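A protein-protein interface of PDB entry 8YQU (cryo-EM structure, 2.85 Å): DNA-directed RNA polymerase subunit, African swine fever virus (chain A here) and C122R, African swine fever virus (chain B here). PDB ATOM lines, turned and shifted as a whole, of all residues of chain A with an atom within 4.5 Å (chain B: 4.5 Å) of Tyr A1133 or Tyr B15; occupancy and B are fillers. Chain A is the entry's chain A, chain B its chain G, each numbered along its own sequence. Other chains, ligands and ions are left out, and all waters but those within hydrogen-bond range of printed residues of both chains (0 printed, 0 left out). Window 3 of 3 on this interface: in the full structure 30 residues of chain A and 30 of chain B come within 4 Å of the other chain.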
ATOM      1  N   LEU A1131      16.249   0.366  22.528  1.00  0.00           N
ATOM      2  CA  LEU A1131      16.390  -1.032  22.922  1.00  0.00           C
ATOM      3  C   LEU A1131      17.578  -1.139  23.872  1.00  0.00           C
ATOM      4  O   LEU A1131      18.716  -0.854  23.488  1.00  0.00           O
ATOM      5  CB  LEU A1131      16.573  -1.928  21.698  1.00  0.00           C
ATOM      6  CG  LEU A1131      16.747  -3.427  21.948  1.00  0.00           C
ATOM      7  CD1 LEU A1131      15.635  -3.963  22.833  1.00  0.00           C
ATOM      8  CD2 LEU A1131      16.794  -4.183  20.632  1.00  0.00           C
ATOM      9  N   LEU A1132      17.312  -1.549  25.109  1.00  0.00           N
ATOM     10  CA  LEU A1132      18.313  -1.571  26.165  1.00  0.00           C
ATOM     11  C   LEU A1132      18.554  -2.997  26.641  1.00  0.00           C
ATOM     12  O   LEU A1132      17.617  -3.792  26.755  1.00  0.00           O
ATOM     13  CB  LEU A1132      17.881  -0.698  27.345  1.00  0.00           C
ATOM     14  CG  LEU A1132      17.378   0.704  27.003  1.00  0.00           C
ATOM     15  CD1 LEU A1132      16.806   1.381  28.237  1.00  0.00           C
ATOM     16  CD2 LEU A1132      18.490   1.541  26.397  1.00  0.00           C
ATOM     17  N   TYR A1133      19.819  -3.312  26.920  1.00  0.00           N
ATOM     18  CA  TYR A1133      20.209  -4.627  27.432  1.00  0.00           C
ATOM     19  C   TYR A1133      20.159  -4.606  28.961  1.00  0.00           C
ATOM     20  O   TYR A1133      21.176  -4.623  29.656  1.00  0.00           O
ATOM     21  CB  TYR A1133      21.594  -5.000  26.919  1.00  0.00           C
ATOM     22  CG  TYR A1133      21.973  -6.448  27.130  1.00  0.00           C
ATOM     23  CD1 TYR A1133      21.500  -7.439  26.282  1.00  0.00           C
ATOM     24  CD2 TYR A1133      22.802  -6.824  28.179  1.00  0.00           C
ATOM     25  CE1 TYR A1133      21.841  -8.763  26.470  1.00  0.00           C
ATOM     26  CE2 TYR A1133      23.148  -8.146  28.375  1.00  0.00           C
ATOM     27  CZ  TYR A1133      22.665  -9.111  27.518  1.00  0.00           C
ATOM     28  OH  TYR A1133      23.007 -10.429  27.709  1.00  0.00           O
ATOM     29  N   GLU A1134      18.935  -4.563  29.485  1.00  0.00           N
ATOM     30  CA  GLU A1134      18.729  -4.389  30.915  1.00  0.00           C
ATOM     31  C   GLU A1134      17.690  -5.368  31.439  1.00  0.00           C
ATOM     32  O   GLU A1134      16.756  -5.744  30.725  1.00  0.00           O
ATOM     33  CB  GLU A1134      18.283  -2.958  31.243  1.00  0.00           C
ATOM     34  CG  GLU A1134      19.257  -1.880  30.810  1.00  0.00           C
ATOM     35  CD  GLU A1134      18.750  -0.488  31.118  1.00  0.00           C
ATOM     36  OE1 GLU A1134      17.647  -0.371  31.692  1.00  0.00           O
ATOM     37  OE2 GLU A1134      19.452   0.490  30.789  1.00  0.00           O
ATOM     38  N   ASN A1173      17.374 -10.056  29.706  1.00  0.00           N
ATOM     39  CA  ASN A1173      18.264  -8.897  29.669  1.00  0.00           C
ATOM     40  C   ASN A1173      17.972  -8.009  28.463  1.00  0.00           C
ATOM     41  O   ASN A1173      18.867  -7.659  27.699  1.00  0.00           O
ATOM     42  CB  ASN A1173      19.713  -9.364  29.662  1.00  0.00           C
ATOM     43  CG  ASN A1173      20.135  -9.972  30.983  1.00  0.00           C
ATOM     44  OD1 ASN A1173      19.815  -9.453  32.052  1.00  0.00           O
ATOM     45  ND2 ASN A1173      20.839 -11.095  30.918  1.00  0.00           N
ATOM     46  N   TRP A1174      16.708  -7.635  28.283  1.00  0.00           N
ATOM     47  CA  TRP A1174      16.306  -6.845  27.128  1.00  0.00           C
ATOM     48  C   TRP A1174      15.191  -5.893  27.529  1.00  0.00           C
ATOM     49  O   TRP A1174      14.162  -6.323  28.057  1.00  0.00           O
ATOM     50  CB  TRP A1174      15.853  -7.747  25.976  1.00  0.00           C
ATOM     51  CG  TRP A1174      16.956  -8.608  25.453  1.00  0.00           C
ATOM     52  CD1 TRP A1174      17.208  -9.906  25.785  1.00  0.00           C
ATOM     53  CD2 TRP A1174      17.972  -8.228  24.520  1.00  0.00           C
ATOM     54  NE1 TRP A1174      18.312 -10.362  25.108  1.00  0.00           N
ATOM     55  CE2 TRP A1174      18.800  -9.350  24.325  1.00  0.00           C
ATOM     56  CE3 TRP A1174      18.259  -7.049  23.826  1.00  0.00           C
ATOM     57  CZ2 TRP A1174      19.895  -9.329  23.465  1.00  0.00           C
ATOM     58  CZ3 TRP A1174      19.346  -7.030  22.974  1.00  0.00           C
ATOM     59  CH2 TRP A1174      20.150  -8.162  22.801  1.00  0.00           C
ATOM     60  N   GLU A1244      19.984 -11.032  20.189  1.00  0.00           N
ATOM     61  CA  GLU A1244      19.780  -9.687  19.664  1.00  0.00           C
ATOM     62  C   GLU A1244      18.808  -9.700  18.489  1.00  0.00           C
ATOM     63  O   GLU A1244      18.071  -8.731  18.275  1.00  0.00           O
ATOM     64  CB  GLU A1244      21.128  -9.083  19.263  1.00  0.00           C
ATOM     65  CG  GLU A1244      21.111  -7.599  18.926  1.00  0.00           C
ATOM     66  CD  GLU A1244      20.708  -7.322  17.492  1.00  0.00           C
ATOM     67  OE1 GLU A1244      20.949  -8.189  16.627  1.00  0.00           O
ATOM     68  OE2 GLU A1244      20.163  -6.230  17.228  1.00  0.00           O
ATOM     69  N   ARG B  13      30.484  -6.332  19.254  1.00  0.00           N
ATOM     70  CA  ARG B  13      29.744  -6.506  20.497  1.00  0.00           C
ATOM     71  C   ARG B  13      28.990  -7.828  20.478  1.00  0.00           C
ATOM     72  O   ARG B  13      28.243  -8.108  19.534  1.00  0.00           O
ATOM     73  CB  ARG B  13      28.760  -5.353  20.702  1.00  0.00           C
ATOM     74  CG  ARG B  13      27.730  -5.601  21.788  1.00  0.00           C
ATOM     75  CD  ARG B  13      26.571  -4.626  21.675  1.00  0.00           C
ATOM     76  NE  ARG B  13      26.861  -3.341  22.299  1.00  0.00           N
ATOM     77  CZ  ARG B  13      26.138  -2.245  22.120  1.00  0.00           C
ATOM     78  NH1 ARG B  13      25.077  -2.238  21.330  1.00  0.00           N
ATOM     79  NH2 ARG B  13      26.488  -1.126  22.749  1.00  0.00           N
ATOM     80  N   THR B  14      29.188  -8.639  21.517  1.00  0.00           N
ATOM     81  CA  THR B  14      28.402  -9.845  21.735  1.00  0.00           C
ATOM     82  C   THR B  14      27.911  -9.852  23.176  1.00  0.00           C
ATOM     83  O   THR B  14      28.275  -8.995  23.987  1.00  0.00           O
ATOM     84  CB  THR B  14      29.200 -11.125  21.430  1.00  0.00           C
ATOM     85  OG1 THR B  14      30.101 -11.404  22.506  1.00  0.00           O
ATOM     86  CG2 THR B  14      29.988 -10.988  20.133  1.00  0.00           C
ATOM     87  N   TYR B  15      27.068 -10.830  23.493  1.00  0.00           N
ATOM     88  CA  TYR B  15      26.397 -10.904  24.785  1.00  0.00           C
ATOM     89  C   TYR B  15      26.691 -12.256  25.414  1.00  0.00           C
ATOM     90  O   TYR B  15      26.379 -13.297  24.825  1.00  0.00           O
ATOM     91  CB  TYR B  15      24.891 -10.704  24.614  1.00  0.00           C
ATOM     92  CG  TYR B  15      24.542  -9.455  23.840  1.00  0.00           C
ATOM     93  CD1 TYR B  15      24.997  -8.210  24.250  1.00  0.00           C
ATOM     94  CD2 TYR B  15      23.783  -9.525  22.680  1.00  0.00           C
ATOM     95  CE1 TYR B  15      24.686  -7.067  23.537  1.00  0.00           C
ATOM     96  CE2 TYR B  15      23.471  -8.390  21.961  1.00  0.00           C
ATOM     97  CZ  TYR B  15      23.925  -7.163  22.394  1.00  0.00           C
ATOM     98  OH  TYR B  15      23.615  -6.029  21.680  1.00  0.00           O
ATOM     99  N   VAL B  16      27.292 -12.246  26.603  1.00  0.00           N
ATOM    100  CA  VAL B  16      27.597 -13.473  27.332  1.00  0.00           C
ATOM    101  C   VAL B  16      27.096 -13.331  28.764  1.00  0.00           C
ATOM    102  O   VAL B  16      27.315 -12.294  29.399  1.00  0.00           O
ATOM    103  CB  VAL B  16      29.103 -13.817  27.295  1.00  0.00           C
ATOM    104  CG1 VAL B  16      29.603 -13.880  25.859  1.00  0.00           C
ATOM    105  CG2 VAL B  16      29.932 -12.810  28.084  1.00  0.00           C
ATOM    106  N   ASP B  17      26.373 -14.347  29.232  1.00  0.00           N
ATOM    107  CA  ASP B  17      25.894 -14.510  30.614  1.00  0.00           C
ATOM    108  C   ASP B  17      25.498 -13.182  31.270  1.00  0.00           C
ATOM    109  O   ASP B  17      25.965 -12.814  32.348  1.00  0.00           O
ATOM    110  CB  ASP B  17      26.900 -15.303  31.465  1.00  0.00           C
ATOM    111  CG  ASP B  17      28.270 -14.633  31.600  1.00  0.00           C
ATOM    112  OD1 ASP B  17      28.406 -13.410  31.424  1.00  0.00           O
ATOM    113  OD2 ASP B  17      29.238 -15.366  31.893  1.00  0.00           O
ATOM    114  N   GLY B  18      24.587 -12.478  30.603  1.00  0.00           N
ATOM    115  CA  GLY B  18      24.057 -11.236  31.137  1.00  0.00           C
ATOM    116  C   GLY B  18      25.034 -10.083  31.170  1.00  0.00           C
ATOM    117  O   GLY B  18      25.026  -9.299  32.125  1.00  0.00           O
ATOM    118  N   ASN B  19      25.876  -9.955  30.148  1.00  0.00           N
ATOM    119  CA  ASN B  19      26.871  -8.897  30.073  1.00  0.00           C
ATOM    120  C   ASN B  19      27.215  -8.646  28.613  1.00  0.00           C
ATOM    121  O   ASN B  19      27.178  -9.558  27.782  1.00  0.00           O
ATOM    122  CB  ASN B  19      28.139  -9.251  30.861  1.00  0.00           C
ATOM    123  CG  ASN B  19      28.039  -8.876  32.324  1.00  0.00           C
ATOM    124  OD1 ASN B  19      27.643  -7.761  32.666  1.00  0.00           O
ATOM    125  ND2 ASN B  19      28.398  -9.807  33.200  1.00  0.00           N
ATOM    126  N   ILE B  20      27.552  -7.395  28.314  1.00  0.00           N
ATOM    127  CA  ILE B  20      27.941  -6.972  26.975  1.00  0.00           C
ATOM    128  C   ILE B  20      29.459  -7.002  26.902  1.00  0.00           C
ATOM    129  O   ILE B  20      30.137  -6.275  27.638  1.00  0.00           O
ATOM    130  CB  ILE B  20      27.401  -5.571  26.650  1.00  0.00           C
ATOM    131  CG1 ILE B  20      25.884  -5.611  26.461  1.00  0.00           C
ATOM    132  CG2 ILE B  20      28.079  -5.011  25.411  1.00  0.00           C
ATOM    133  CD1 ILE B  20      25.274  -4.268  26.133  1.00  0.00           C
ATOM    134  N   LEU B  37      24.972   0.139  26.876  1.00  0.00           N
ATOM    135  CA  LEU B  37      23.711  -0.596  26.966  1.00  0.00           C
ATOM    136  C   LEU B  37      22.650   0.006  26.048  1.00  0.00           C
ATOM    137  O   LEU B  37      21.529   0.292  26.465  1.00  0.00           O
ATOM    138  CB  LEU B  37      23.229  -0.622  28.410  1.00  0.00           C
ATOM    139  CG  LEU B  37      24.116  -1.328  29.434  1.00  0.00           C
ATOM    140  CD1 LEU B  37      23.806  -0.822  30.830  1.00  0.00           C
ATOM    141  CD2 LEU B  37      23.929  -2.833  29.355  1.00  0.00           C
ATOM    142  N   VAL B  39      21.398  -1.087  22.385  1.00  0.00           N
ATOM    143  CA  VAL B  39      21.490  -1.987  21.240  1.00  0.00           C
ATOM    144  C   VAL B  39      21.097  -1.265  19.956  1.00  0.00           C
ATOM    145  O   VAL B  39      21.811  -1.325  18.947  1.00  0.00           O
ATOM    146  CB  VAL B  39      20.621  -3.236  21.473  1.00  0.00           C
ATOM    147  CG1 VAL B  39      20.723  -4.179  20.287  1.00  0.00           C
ATOM    148  CG2 VAL B  39      21.037  -3.931  22.759  1.00  0.00           C
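Among the printed residues, merely in contact across the chains: Leu A1132 with Leu B37, Tyr A1133 with Tyr B15, Tyr A1133 with Gly B18, Tyr A1133 with Asn B19, Tyr A1133 with Ile B20, Tyr A1133 with Leu B37, Asn A1173 with Gly B18, Trp A1174 with Tyr B15, Trp A1174 with Val B39, Glu A1244 with Tyr B15 and Glu A1244 with Val B39.
Hydrophobic or aromatic side chains of chain A that line the printed part of chain B: Leu A1131, Leu A1132, Tyr A1133 and Trp A1174.
Of the 10 printed residues of chain B, 6 touch a printed residue of chain A.
Printed residues of chain B that touch a printed residue of chain A: Tyr B15, Gly B18, Asn B19, Ile B20, Leu B37 and Val B39.
Among the printed residues, 12 pairs touch across the chains.
Among the printed residues, no Asp or Glu carboxylate lies within 4 Å of a Lys or Arg side-chain nitrogen of the other chain.
The backbone carbonyl oxygen (O) of Leu A1131 sits at hydrogen-bond distance from the backbone NH (N) of Val B39, 2.9 Å away.
The backbone NH of Trp A1174 lies within hydrogen-bond range of the backbone carbonyl oxygen of Glu A1134, at 3.1 Å.
Tyr A1133 touches just these residues of chain B: Tyr B15, Gly B18, Asn B19, Ile B20 and Leu B37.
Tyr B15 touches three residues of chain A.
Of the printed residues of chain B, Leu A1132 touches Leu B37.
Of the printed residues of chain B, Leu A1131 touches Val B39.
Printed residues of chain A within 4 Å of Val B39: Leu A1131, Trp A1174 and Glu A1244.
Of the printed residues of chain A, Ile B20 touches Tyr A1133.
Arg B13 touches none of the printed residues of chain A.
The nearest printed residue of chain A that does not touch Tyr B15 is Asn A1173 (7.1 Å).
The nearest printed residue of chain B that does not touch Glu A1244 is Arg B13 (6.8 Å).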
